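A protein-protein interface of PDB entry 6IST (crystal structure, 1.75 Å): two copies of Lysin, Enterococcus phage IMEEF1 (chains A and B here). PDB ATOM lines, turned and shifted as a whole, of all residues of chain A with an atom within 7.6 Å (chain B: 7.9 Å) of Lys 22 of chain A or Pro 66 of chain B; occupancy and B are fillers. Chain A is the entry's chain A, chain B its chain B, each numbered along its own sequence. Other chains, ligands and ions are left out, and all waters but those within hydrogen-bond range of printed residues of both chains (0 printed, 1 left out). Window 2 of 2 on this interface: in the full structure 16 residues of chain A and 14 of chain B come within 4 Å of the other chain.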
ATOM      1  N   MET A   1      -9.424  18.277 -14.188  1.00  0.00           N
ATOM      2  CA  MET A   1     -10.235  19.462 -14.407  1.00  0.00           C
ATOM      3  C   MET A   1      -9.682  20.562 -13.536  1.00  0.00           C
ATOM      4  O   MET A   1      -9.588  20.369 -12.343  1.00  0.00           O
ATOM      5  CB  MET A   1     -11.642  19.268 -13.899  1.00  0.00           C
ATOM      6  CG  MET A   1     -12.629  18.649 -14.853  1.00  0.00           C
ATOM      7  SD  MET A   1     -14.332  18.668 -14.194  1.00  0.00           S
ATOM      8  CE  MET A   1     -14.322  20.255 -13.586  1.00  0.00           C
ATOM      9  N   PHE A   2      -9.391  21.719 -14.120  1.00  0.00           N
ATOM     10  CA  PHE A   2      -9.027  22.904 -13.369  1.00  0.00           C
ATOM     11  C   PHE A   2      -9.089  24.181 -14.233  1.00  0.00           C
ATOM     12  O   PHE A   2      -9.236  24.089 -15.426  1.00  0.00           O
ATOM     13  CB  PHE A   2      -7.661  22.765 -12.684  1.00  0.00           C
ATOM     14  CG  PHE A   2      -6.508  22.523 -13.618  1.00  0.00           C
ATOM     15  CD1 PHE A   2      -5.851  23.576 -14.195  1.00  0.00           C
ATOM     16  CD2 PHE A   2      -6.191  21.221 -14.008  1.00  0.00           C
ATOM     17  CE1 PHE A   2      -4.780  23.329 -15.038  1.00  0.00           C
ATOM     18  CE2 PHE A   2      -5.121  20.961 -14.829  1.00  0.00           C
ATOM     19  CZ  PHE A   2      -4.432  22.019 -15.378  1.00  0.00           C
ATOM     20  N   TYR A   4      -7.086  27.874 -15.095  1.00  0.00           N
ATOM     21  CA  TYR A   4      -5.958  28.743 -14.907  1.00  0.00           C
ATOM     22  C   TYR A   4      -6.164  30.094 -15.620  1.00  0.00           C
ATOM     23  O   TYR A   4      -7.019  30.205 -16.485  1.00  0.00           O
ATOM     24  CB  TYR A   4      -4.664  28.092 -15.400  1.00  0.00           C
ATOM     25  CG  TYR A   4      -4.619  27.802 -16.885  1.00  0.00           C
ATOM     26  CD1 TYR A   4      -4.113  28.742 -17.771  1.00  0.00           C
ATOM     27  CD2 TYR A   4      -4.983  26.532 -17.396  1.00  0.00           C
ATOM     28  CE1 TYR A   4      -4.053  28.475 -19.110  1.00  0.00           C
ATOM     29  CE2 TYR A   4      -4.912  26.254 -18.754  1.00  0.00           C
ATOM     30  CZ  TYR A   4      -4.416  27.228 -19.597  1.00  0.00           C
ATOM     31  OH  TYR A   4      -4.359  26.983 -20.949  1.00  0.00           O
ATOM     32  N   TRP A  16      -8.901  30.023 -18.608  1.00  0.00           N
ATOM     33  CA  TRP A  16      -8.945  28.784 -19.356  1.00  0.00           C
ATOM     34  C   TRP A  16      -9.339  27.610 -18.477  1.00  0.00           C
ATOM     35  O   TRP A  16      -8.947  27.550 -17.361  1.00  0.00           O
ATOM     36  CB  TRP A  16      -7.565  28.523 -19.927  1.00  0.00           C
ATOM     37  CG  TRP A  16      -7.163  29.451 -21.008  1.00  0.00           C
ATOM     38  CD1 TRP A  16      -6.726  30.727 -20.890  1.00  0.00           C
ATOM     39  CD2 TRP A  16      -7.213  29.167 -22.407  1.00  0.00           C
ATOM     40  NE1 TRP A  16      -6.465  31.270 -22.138  1.00  0.00           N
ATOM     41  CE2 TRP A  16      -6.792  30.348 -23.090  1.00  0.00           C
ATOM     42  CE3 TRP A  16      -7.617  28.056 -23.145  1.00  0.00           C
ATOM     43  CZ2 TRP A  16      -6.695  30.409 -24.480  1.00  0.00           C
ATOM     44  CZ3 TRP A  16      -7.555  28.109 -24.504  1.00  0.00           C
ATOM     45  CH2 TRP A  16      -7.072  29.268 -25.178  1.00  0.00           C
ATOM     46  N   PHE A  17     -10.040  26.653 -19.060  1.00  0.00           N
ATOM     47  CA  PHE A  17     -10.623  25.519 -18.341  1.00  0.00           C
ATOM     48  C   PHE A  17     -10.025  24.269 -18.938  1.00  0.00           C
ATOM     49  O   PHE A  17     -10.110  24.087 -20.108  1.00  0.00           O
ATOM     50  CB  PHE A  17     -12.142  25.509 -18.492  1.00  0.00           C
ATOM     51  CG  PHE A  17     -12.849  24.417 -17.745  1.00  0.00           C
ATOM     52  CD1 PHE A  17     -12.403  23.966 -16.512  1.00  0.00           C
ATOM     53  CD2 PHE A  17     -13.950  23.789 -18.321  1.00  0.00           C
ATOM     54  CE1 PHE A  17     -13.079  22.981 -15.849  1.00  0.00           C
ATOM     55  CE2 PHE A  17     -14.649  22.795 -17.637  1.00  0.00           C
ATOM     56  CZ  PHE A  17     -14.178  22.363 -16.423  1.00  0.00           C
ATOM     57  N   VAL A  18      -9.370  23.472 -18.099  1.00  0.00           N
ATOM     58  CA  VAL A  18      -8.796  22.175 -18.523  1.00  0.00           C
ATOM     59  C   VAL A  18      -9.746  21.083 -18.171  1.00  0.00           C
ATOM     60  O   VAL A  18     -10.176  20.972 -17.030  1.00  0.00           O
ATOM     61  CB  VAL A  18      -7.408  21.961 -17.869  1.00  0.00           C
ATOM     62  CG1 VAL A  18      -6.898  20.544 -18.202  1.00  0.00           C
ATOM     63  CG2 VAL A  18      -6.435  22.970 -18.423  1.00  0.00           C
ATOM     64  N   ILE A  19     -10.166  20.311 -19.172  1.00  0.00           N
ATOM     65  CA  ILE A  19     -11.119  19.242 -18.971  1.00  0.00           C
ATOM     66  C   ILE A  19     -10.917  18.214 -20.051  1.00  0.00           C
ATOM     67  O   ILE A  19     -10.657  18.587 -21.215  1.00  0.00           O
ATOM     68  CB  ILE A  19     -12.581  19.769 -18.983  1.00  0.00           C
ATOM     69  CG1 ILE A  19     -13.587  18.604 -18.823  1.00  0.00           C
ATOM     70  CG2 ILE A  19     -12.872  20.554 -20.255  1.00  0.00           C
ATOM     71  CD1 ILE A  19     -14.978  18.981 -18.360  1.00  0.00           C
ATOM     72  N   GLY A  20     -10.988  16.934 -19.687  1.00  0.00           N
ATOM     73  CA  GLY A  20     -10.898  15.856 -20.663  1.00  0.00           C
ATOM     74  C   GLY A  20      -9.651  15.884 -21.539  1.00  0.00           C
ATOM     75  O   GLY A  20      -9.701  15.498 -22.729  1.00  0.00           O
ATOM     76  N   GLY A  21      -8.538  16.349 -20.989  1.00  0.00           N
ATOM     77  CA  GLY A  21      -7.328  16.517 -21.760  1.00  0.00           C
ATOM     78  C   GLY A  21      -7.306  17.629 -22.762  1.00  0.00           C
ATOM     79  O   GLY A  21      -6.420  17.649 -23.627  1.00  0.00           O
ATOM     80  N   LYS A  22      -8.251  18.565 -22.653  1.00  0.00           N
ATOM     81  CA  LYS A  22      -8.413  19.660 -23.612  1.00  0.00           C
ATOM     82  C   LYS A  22      -8.434  20.968 -22.830  1.00  0.00           C
ATOM     83  O   LYS A  22      -8.582  20.932 -21.627  1.00  0.00           O
ATOM     84  CB  LYS A  22      -9.715  19.579 -24.416  1.00  0.00           C
ATOM     85  CG  LYS A  22     -10.061  18.217 -24.955  1.00  0.00           C
ATOM     86  CD  LYS A  22      -9.226  17.799 -26.122  1.00  0.00           C
ATOM     87  CE  LYS A  22      -9.406  16.314 -26.440  1.00  0.00           C
ATOM     88  NZ  LYS A  22     -10.783  15.746 -26.549  1.00  0.00           N
ATOM     89  N   ARG A  23      -8.294  22.078 -23.534  1.00  0.00           N
ATOM     90  CA  ARG A  23      -8.305  23.443 -22.942  1.00  0.00           C
ATOM     91  C   ARG A  23      -9.432  24.188 -23.576  1.00  0.00           C
ATOM     92  O   ARG A  23      -9.525  24.179 -24.776  1.00  0.00           O
ATOM     93  CB  ARG A  23      -7.082  24.231 -23.351  1.00  0.00           C
ATOM     94  CG  ARG A  23      -5.865  23.890 -22.594  1.00  0.00           C
ATOM     95  CD  ARG A  23      -4.676  24.705 -23.103  1.00  0.00           C
ATOM     96  NE  ARG A  23      -4.325  24.431 -24.481  1.00  0.00           N
ATOM     97  CZ  ARG A  23      -4.214  25.314 -25.467  1.00  0.00           C
ATOM     98  NH1 ARG A  23      -4.408  26.628 -25.305  1.00  0.00           N
ATOM     99  NH2 ARG A  23      -3.891  24.849 -26.656  1.00  0.00           N
ATOM    100  N   ILE A  24     -10.215  24.912 -22.775  1.00  0.00           N
ATOM    101  CA  ILE A  24     -11.287  25.708 -23.299  1.00  0.00           C
ATOM    102  C   ILE A  24     -11.120  27.136 -22.788  1.00  0.00           C
ATOM    103  O   ILE A  24     -11.052  27.346 -21.593  1.00  0.00           O
ATOM    104  CB  ILE A  24     -12.685  25.174 -22.862  1.00  0.00           C
ATOM    105  CG1 ILE A  24     -12.936  23.738 -23.388  1.00  0.00           C
ATOM    106  CG2 ILE A  24     -13.802  26.121 -23.376  1.00  0.00           C
ATOM    107  CD1 ILE A  24     -14.243  23.133 -22.881  1.00  0.00           C
ATOM    108  N   MET A  61       1.557  22.872 -21.042  1.00  0.00           N
ATOM    109  CA  MET A  61       0.109  22.607 -21.041  1.00  0.00           C
ATOM    110  C   MET A  61      -0.495  22.914 -22.426  1.00  0.00           C
ATOM    111  O   MET A  61      -1.288  22.105 -22.940  1.00  0.00           O
ATOM    112  CB  MET A  61      -0.619  23.429 -19.989  1.00  0.00           C
ATOM    113  CG  MET A  61      -0.333  23.011 -18.538  1.00  0.00           C
ATOM    114  SD  MET A  61      -1.515  23.740 -17.255  1.00  0.00           S
ATOM    115  CE  MET A  61      -0.848  25.374 -17.211  1.00  0.00           C
ATOM    116  N   ALA A  64       0.298  20.117 -24.898  1.00  0.00           N
ATOM    117  CA  ALA A  64      -0.185  18.808 -24.601  1.00  0.00           C
ATOM    118  C   ALA A  64      -1.730  18.720 -24.621  1.00  0.00           C
ATOM    119  O   ALA A  64      -2.285  17.635 -24.761  1.00  0.00           O
ATOM    120  CB  ALA A  64       0.324  18.327 -23.233  1.00  0.00           C
ATOM    121  N   LEU A  65      -2.410  19.861 -24.424  1.00  0.00           N
ATOM    122  CA  LEU A  65      -3.834  19.888 -24.236  1.00  0.00           C
ATOM    123  C   LEU A  65      -4.385  20.709 -25.393  1.00  0.00           C
ATOM    124  O   LEU A  65      -4.381  21.916 -25.329  1.00  0.00           O
ATOM    125  CB  LEU A  65      -4.166  20.546 -22.884  1.00  0.00           C
ATOM    126  CG  LEU A  65      -3.572  19.886 -21.628  1.00  0.00           C
ATOM    127  CD1 LEU A  65      -3.668  20.824 -20.424  1.00  0.00           C
ATOM    128  CD2 LEU A  65      -4.198  18.554 -21.328  1.00  0.00           C
ATOM    129  N   PRO A  66      -4.902  20.041 -26.443  1.00  0.00           N
ATOM    130  CA  PRO A  66      -5.480  20.788 -27.571  1.00  0.00           C
ATOM    131  C   PRO A  66      -6.592  21.711 -27.140  1.00  0.00           C
ATOM    132  O   PRO A  66      -7.379  21.360 -26.268  1.00  0.00           O
ATOM    133  CB  PRO A  66      -6.077  19.683 -28.458  1.00  0.00           C
ATOM    134  CG  PRO A  66      -5.339  18.442 -28.065  1.00  0.00           C
ATOM    135  CD  PRO A  66      -5.015  18.582 -26.621  1.00  0.00           C
ATOM    136  N   GLN A  67      -6.718  22.844 -27.810  1.00  0.00           N
ATOM    137  CA  GLN A  67      -7.860  23.763 -27.558  1.00  0.00           C
ATOM    138  C   GLN A  67      -9.136  23.245 -28.228  1.00  0.00           C
ATOM    139  O   GLN A  67      -9.095  22.853 -29.363  1.00  0.00           O
ATOM    140  CB  GLN A  67      -7.592  25.164 -28.132  1.00  0.00           C
ATOM    141  CG  GLN A  67      -8.675  26.178 -27.814  1.00  0.00           C
ATOM    142  CD  GLN A  67      -8.356  27.645 -28.216  1.00  0.00           C
ATOM    143  OE1 GLN A  67      -9.156  28.557 -27.932  1.00  0.00           O
ATOM    144  NE2 GLN A  67      -7.219  27.862 -28.864  1.00  0.00           N
ATOM    145  N   VAL A  68     -10.269  23.319 -27.557  1.00  0.00           N
ATOM    146  CA  VAL A  68     -11.585  23.113 -28.228  1.00  0.00           C
ATOM    147  C   VAL A  68     -12.427  24.327 -27.943  1.00  0.00           C
ATOM    148  O   VAL A  68     -12.258  24.977 -26.925  1.00  0.00           O
ATOM    149  CB  VAL A  68     -12.334  21.859 -27.792  1.00  0.00           C
ATOM    150  CG1 VAL A  68     -11.556  20.591 -28.144  1.00  0.00           C
ATOM    151  CG2 VAL A  68     -12.660  21.876 -26.328  1.00  0.00           C
ATOM    152  N   TRP B  16     -25.677   9.453 -19.899  1.00  0.00           N
ATOM    153  CA  TRP B  16     -24.423   9.468 -20.597  1.00  0.00           C
ATOM    154  C   TRP B  16     -23.333   9.059 -19.597  1.00  0.00           C
ATOM    155  O   TRP B  16     -23.406   9.436 -18.440  1.00  0.00           O
ATOM    156  CB  TRP B  16     -24.138  10.869 -21.132  1.00  0.00           C
ATOM    157  CG  TRP B  16     -24.953  11.223 -22.303  1.00  0.00           C
ATOM    158  CD1 TRP B  16     -26.240  11.698 -22.311  1.00  0.00           C
ATOM    159  CD2 TRP B  16     -24.532  11.177 -23.651  1.00  0.00           C
ATOM    160  NE1 TRP B  16     -26.639  11.955 -23.597  1.00  0.00           N
ATOM    161  CE2 TRP B  16     -25.623  11.617 -24.444  1.00  0.00           C
ATOM    162  CE3 TRP B  16     -23.355  10.745 -24.275  1.00  0.00           C
ATOM    163  CZ2 TRP B  16     -25.558  11.709 -25.813  1.00  0.00           C
ATOM    164  CZ3 TRP B  16     -23.278  10.851 -25.651  1.00  0.00           C
ATOM    165  CH2 TRP B  16     -24.376  11.351 -26.405  1.00  0.00           C
ATOM    166  N   PHE B  17     -22.338   8.331 -20.077  1.00  0.00           N
ATOM    167  CA  PHE B  17     -21.253   7.806 -19.261  1.00  0.00           C
ATOM    168  C   PHE B  17     -19.956   8.410 -19.785  1.00  0.00           C
ATOM    169  O   PHE B  17     -19.692   8.383 -20.970  1.00  0.00           O
ATOM    170  CB  PHE B  17     -21.227   6.278 -19.384  1.00  0.00           C
ATOM    171  CG  PHE B  17     -20.128   5.610 -18.647  1.00  0.00           C
ATOM    172  CD1 PHE B  17     -19.761   6.016 -17.385  1.00  0.00           C
ATOM    173  CD2 PHE B  17     -19.512   4.481 -19.190  1.00  0.00           C
ATOM    174  CE1 PHE B  17     -18.766   5.357 -16.728  1.00  0.00           C
ATOM    175  CE2 PHE B  17     -18.526   3.802 -18.513  1.00  0.00           C
ATOM    176  CZ  PHE B  17     -18.147   4.239 -17.277  1.00  0.00           C
ATOM    177  N   VAL B  18     -19.172   8.999 -18.885  1.00  0.00           N
ATOM    178  CA  VAL B  18     -17.860   9.567 -19.237  1.00  0.00           C
ATOM    179  C   VAL B  18     -16.775   8.627 -18.797  1.00  0.00           C
ATOM    180  O   VAL B  18     -16.715   8.264 -17.626  1.00  0.00           O
ATOM    181  CB  VAL B  18     -17.613  10.951 -18.592  1.00  0.00           C
ATOM    182  CG1 VAL B  18     -16.167  11.464 -18.924  1.00  0.00           C
ATOM    183  CG2 VAL B  18     -18.694  11.898 -19.090  1.00  0.00           C
ATOM    184  N   ILE B  19     -15.928   8.239 -19.754  1.00  0.00           N
ATOM    185  CA  ILE B  19     -14.863   7.277 -19.487  1.00  0.00           C
ATOM    186  C   ILE B  19     -13.753   7.476 -20.509  1.00  0.00           C
ATOM    187  O   ILE B  19     -14.029   7.620 -21.690  1.00  0.00           O
ATOM    188  CB  ILE B  19     -15.375   5.814 -19.511  1.00  0.00           C
ATOM    189  CG1 ILE B  19     -14.207   4.817 -19.497  1.00  0.00           C
ATOM    190  CG2 ILE B  19     -16.237   5.506 -20.744  1.00  0.00           C
ATOM    191  CD1 ILE B  19     -14.625   3.394 -19.186  1.00  0.00           C
ATOM    192  N   GLY B  20     -12.510   7.505 -20.025  1.00  0.00           N
ATOM    193  CA  GLY B  20     -11.338   7.609 -20.938  1.00  0.00           C
ATOM    194  C   GLY B  20     -11.331   8.883 -21.752  1.00  0.00           C
ATOM    195  O   GLY B  20     -10.876   8.903 -22.884  1.00  0.00           O
ATOM    196  N   GLY B  21     -11.869   9.965 -21.193  1.00  0.00           N
ATOM    197  CA  GLY B  21     -11.974  11.207 -21.945  1.00  0.00           C
ATOM    198  C   GLY B  21     -13.024  11.185 -23.044  1.00  0.00           C
ATOM    199  O   GLY B  21     -13.024  12.069 -23.874  1.00  0.00           O
ATOM    200  N   LYS B  22     -13.894  10.186 -23.051  1.00  0.00           N
ATOM    201  CA  LYS B  22     -14.942  10.041 -24.037  1.00  0.00           C
ATOM    202  C   LYS B  22     -16.304  10.004 -23.373  1.00  0.00           C
ATOM    203  O   LYS B  22     -16.413   9.797 -22.180  1.00  0.00           O
ATOM    204  CB  LYS B  22     -14.827   8.692 -24.753  1.00  0.00           C
ATOM    205  CG  LYS B  22     -13.479   8.311 -25.281  1.00  0.00           C
ATOM    206  CD  LYS B  22     -13.102   9.143 -26.467  1.00  0.00           C
ATOM    207  CE  LYS B  22     -11.585   9.074 -26.664  1.00  0.00           C
ATOM    208  NZ  LYS B  22     -11.086   7.690 -26.853  1.00  0.00           N
ATOM    209  N   ARG B  23     -17.374  10.176 -24.160  1.00  0.00           N
ATOM    210  CA  ARG B  23     -18.712  10.023 -23.611  1.00  0.00           C
ATOM    211  C   ARG B  23     -19.534   9.010 -24.417  1.00  0.00           C
ATOM    212  O   ARG B  23     -19.409   8.918 -25.618  1.00  0.00           O
ATOM    213  CB  ARG B  23     -19.443  11.353 -23.417  1.00  0.00           C
ATOM    214  CG  ARG B  23     -19.785  12.114 -24.658  1.00  0.00           C
ATOM    215  CD  ARG B  23     -20.054  13.617 -24.340  1.00  0.00           C
ATOM    216  NE  ARG B  23     -19.837  14.306 -25.606  1.00  0.00           N
ATOM    217  CZ  ARG B  23     -20.738  14.385 -26.570  1.00  0.00           C
ATOM    218  NH1 ARG B  23     -21.956  13.967 -26.385  1.00  0.00           N
ATOM    219  NH2 ARG B  23     -20.432  14.964 -27.693  1.00  0.00           N
ATOM    220  N   ILE B  24     -20.334   8.240 -23.698  1.00  0.00           N
ATOM    221  CA  ILE B  24     -21.082   7.110 -24.282  1.00  0.00           C
ATOM    222  C   ILE B  24     -22.525   7.275 -23.864  1.00  0.00           C
ATOM    223  O   ILE B  24     -22.823   7.337 -22.680  1.00  0.00           O
ATOM    224  CB  ILE B  24     -20.568   5.757 -23.764  1.00  0.00           C
ATOM    225  CG1 ILE B  24     -19.053   5.659 -24.082  1.00  0.00           C
ATOM    226  CG2 ILE B  24     -21.405   4.599 -24.371  1.00  0.00           C
ATOM    227  CD1 ILE B  24     -18.445   4.338 -23.671  1.00  0.00           C
ATOM    228  N   MET B  60     -19.665  22.464 -22.656  1.00  0.00           N
ATOM    229  CA  MET B  60     -18.202  22.343 -22.545  1.00  0.00           C
ATOM    230  C   MET B  60     -17.827  20.872 -22.487  1.00  0.00           C
ATOM    231  O   MET B  60     -16.904  20.458 -23.192  1.00  0.00           O
ATOM    232  CB  MET B  60     -17.632  23.167 -21.351  1.00  0.00           C
ATOM    233  CG  MET B  60     -17.739  24.708 -21.555  1.00  0.00           C
ATOM    234  SD  MET B  60     -16.881  25.681 -20.285  1.00  0.00           S
ATOM    235  CE  MET B  60     -18.039  25.538 -18.960  1.00  0.00           C
ATOM    236  N   MET B  61     -18.545  20.065 -21.686  1.00  0.00           N
ATOM    237  CA  MET B  61     -18.277  18.635 -21.651  1.00  0.00           C
ATOM    238  C   MET B  61     -18.429  18.029 -23.045  1.00  0.00           C
ATOM    239  O   MET B  61     -17.591  17.229 -23.457  1.00  0.00           O
ATOM    240  CB  MET B  61     -19.193  17.881 -20.637  1.00  0.00           C
ATOM    241  CG  MET B  61     -18.810  18.127 -19.200  1.00  0.00           C
ATOM    242  SD  MET B  61     -19.582  16.971 -17.985  1.00  0.00           S
ATOM    243  CE  MET B  61     -21.279  17.502 -18.129  1.00  0.00           C
ATOM    244  N   GLU B  62     -19.456  18.452 -23.774  1.00  0.00           N
ATOM    245  CA  GLU B  62     -19.780  17.834 -25.051  1.00  0.00           C
ATOM    246  C   GLU B  62     -18.748  18.216 -26.088  1.00  0.00           C
ATOM    247  O   GLU B  62     -18.414  17.399 -26.960  1.00  0.00           O
ATOM    248  CB  GLU B  62     -21.205  18.212 -25.553  1.00  0.00           C
ATOM    249  CG  GLU B  62     -22.283  17.351 -24.916  1.00  0.00           C
ATOM    250  CD  GLU B  62     -23.733  17.793 -25.212  1.00  0.00           C
ATOM    251  OE1 GLU B  62     -24.649  16.966 -25.024  1.00  0.00           O
ATOM    252  OE2 GLU B  62     -23.987  18.983 -25.573  1.00  0.00           O
ATOM    253  N   ALA B  63     -18.206  19.409 -25.965  1.00  0.00           N
ATOM    254  CA  ALA B  63     -17.068  19.791 -26.835  1.00  0.00           C
ATOM    255  C   ALA B  63     -15.743  19.095 -26.515  1.00  0.00           C
ATOM    256  O   ALA B  63     -14.890  18.912 -27.380  1.00  0.00           O
ATOM    257  CB  ALA B  63     -16.891  21.296 -26.795  1.00  0.00           C
ATOM    258  N   ALA B  64     -15.482  18.840 -25.245  1.00  0.00           N
ATOM    259  CA  ALA B  64     -14.189  18.350 -24.855  1.00  0.00           C
ATOM    260  C   ALA B  64     -14.139  16.824 -24.931  1.00  0.00           C
ATOM    261  O   ALA B  64     -13.050  16.271 -25.141  1.00  0.00           O
ATOM    262  CB  ALA B  64     -13.834  18.813 -23.483  1.00  0.00           C
ATOM    263  N   LEU B  65     -15.289  16.161 -24.771  1.00  0.00           N
ATOM    264  CA  LEU B  65     -15.352  14.716 -24.688  1.00  0.00           C
ATOM    265  C   LEU B  65     -16.049  14.156 -25.938  1.00  0.00           C
ATOM    266  O   LEU B  65     -17.258  14.158 -25.995  1.00  0.00           O
ATOM    267  CB  LEU B  65     -16.128  14.318 -23.417  1.00  0.00           C
ATOM    268  CG  LEU B  65     -15.601  14.968 -22.152  1.00  0.00           C
ATOM    269  CD1 LEU B  65     -16.623  14.757 -21.041  1.00  0.00           C
ATOM    270  CD2 LEU B  65     -14.244  14.421 -21.764  1.00  0.00           C
ATOM    271  N   PRO B  66     -15.285  13.651 -26.924  1.00  0.00           N
ATOM    272  CA  PRO B  66     -15.938  13.042 -28.074  1.00  0.00           C
ATOM    273  C   PRO B  66     -16.841  11.850 -27.735  1.00  0.00           C
ATOM    274  O   PRO B  66     -16.576  11.042 -26.805  1.00  0.00           O
ATOM    275  CB  PRO B  66     -14.749  12.487 -28.922  1.00  0.00           C
ATOM    276  CG  PRO B  66     -13.505  12.987 -28.264  1.00  0.00           C
ATOM    277  CD  PRO B  66     -13.868  13.240 -26.833  1.00  0.00           C
ATOM    278  N   GLN B  67     -17.855  11.674 -28.570  1.00  0.00           N
ATOM    279  CA  GLN B  67     -18.785  10.621 -28.396  1.00  0.00           C
ATOM    280  C   GLN B  67     -18.211   9.371 -29.003  1.00  0.00           C
ATOM    281  O   GLN B  67     -17.629   9.401 -30.076  1.00  0.00           O
ATOM    282  CB  GLN B  67     -20.109  10.948 -29.074  1.00  0.00           C
ATOM    283  CG  GLN B  67     -21.042   9.759 -28.993  1.00  0.00           C
ATOM    284  CD  GLN B  67     -22.439  10.033 -29.440  1.00  0.00           C
ATOM    285  OE1 GLN B  67     -22.747  11.142 -29.923  1.00  0.00           O
ATOM    286  NE2 GLN B  67     -23.319   9.055 -29.217  1.00  0.00           N
ATOM    287  N   VAL B  68     -18.340   8.270 -28.297  1.00  0.00           N
ATOM    288  CA  VAL B  68     -18.122   6.970 -28.937  1.00  0.00           C
ATOM    289  C   VAL B  68     -19.350   6.126 -28.759  1.00  0.00           C
ATOM    290  O   VAL B  68     -20.126   6.291 -27.811  1.00  0.00           O
ATOM    291  CB  VAL B  68     -16.859   6.221 -28.445  1.00  0.00           C
ATOM    292  CG1 VAL B  68     -15.612   7.099 -28.605  1.00  0.00           C
ATOM    293  CG2 VAL B  68     -17.025   5.755 -27.022  1.00  0.00           C
ATOM    294  N   LYS B  69     -19.486   5.177 -29.666  1.00  0.00           N
ATOM    295  CA  LYS B  69     -20.747   4.505 -29.878  1.00  0.00           C
ATOM    296  C   LYS B  69     -20.782   3.114 -29.288  1.00  0.00           C
ATOM    297  O   LYS B  69     -19.874   2.314 -29.478  1.00  0.00           O
ATOM    298  CB  LYS B  69     -21.033   4.404 -31.368  1.00  0.00           C
ATOM    299  CG  LYS B  69     -22.462   4.696 -31.733  1.00  0.00           C
ATOM    300  CD  LYS B  69     -22.684   6.161 -32.020  1.00  0.00           C
ATOM    301  CE  LYS B  69     -23.930   6.268 -32.876  1.00  0.00           C
ATOM    302  NZ  LYS B  69     -24.384   7.662 -33.028  1.00  0.00           N
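Among the printed residues, pairs that only touch across the chains: Ile 19 of chain A with Ala 64 of chain B, Gly 20 of chain A with Leu 65 of chain B, Lys 22 of chain A with Pro 66 of chain B, Ile 24 of chain A with Met 60 of chain B and Val 68 of chain A with Ala 63 of chain B.
Ile 19 of chain A touches Ala 64 of chain B, but with the chains exchanged Ala 64 of chain A does not touch Ile 19 of chain B (15.7 Å). Gly 20 of chain A touches Leu 65 of chain B, but with the chains exchanged Leu 65 of chain A does not touch Gly 20 of chain B (11.8 Å). Lys 22 of chain A touches Ala 64 of chain B, but with the chains exchanged Ala 64 of chain A does not touch Lys 22 of chain B (12.8 Å). Lys 22 of chain A touches Pro 66 of chain B, but with the chains exchanged Pro 66 of chain A does not touch Lys 22 of chain B (11.3 Å). Positions printed for both chains: 16, 17, 18, 19, 20, 21, 22, 23, 24, 61, 64, 65, 66, 67 and 68. Of the 6 pairs that touch across the chains among the printed residues, none has its exchanged pair printed and touching as well.
The backbone carbonyl oxygen of Phe 17 of chain A is in hydrogen-bond range of the backbone NH of Ile 24 of chain A (2.8 Å). The backbone carbonyl oxygen of Arg 23 of chain A lies within hydrogen-bond range of the backbone NH of Val 68 of chain A (3.0 Å). The guanidinium group (NE) of Arg 23 of chain B lies within hydrogen-bond range of the backbone carbonyl oxygen (O) of Leu 65 of chain B, 2.6 Å away. The backbone carbonyl oxygen (O) of Pro 66 of chain B sits at hydrogen-bond distance from the backbone NH (N) of Arg 23 of chain B.
Of the 18 printed residues of chain A, 5 touch a printed residue of chain B. Printed residues of chain A that touch a printed residue of chain B: Ile 19, Gly 20, Lys 22, Ile 24 and Val 68. Hydrophobic or aromatic side chains of chain A within 4 Å of the printed part of chain B: Ile 19, Ile 24 and Val 68.
Printed residues of chain B within 4 Å of Lys 22 of chain A: Ala 64 (2.7 Å) and Pro 66 (3.98 Å). Of the printed residues of chain A, Pro 66 of chain B touches Lys 22 (3.98 Å). No residue of chain B comes within 4 Å of Gly 21 of chain A. Of the printed residues of chain A, Ala 64 of chain B touches Ile 19 (3.8 Å) and Lys 22 (2.7 Å). Of the printed residues of chain B, Val 68 of chain A touches Ala 63 (3.8 Å). Met 61 of chain B touches none of the printed residues of chain A. The nearest printed residue of chain B that does not touch Lys 22 of chain A is Leu 65 of chain B (4.9 Å). The nearest printed residue of chain A that does not touch Ala 64 of chain B is Val 68 of chain A (4.1 Å).
NZ of Lys 22 of chain A lies within hydrogen-bond range of O of Ala 64 of chain B, 2.7 Å away.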
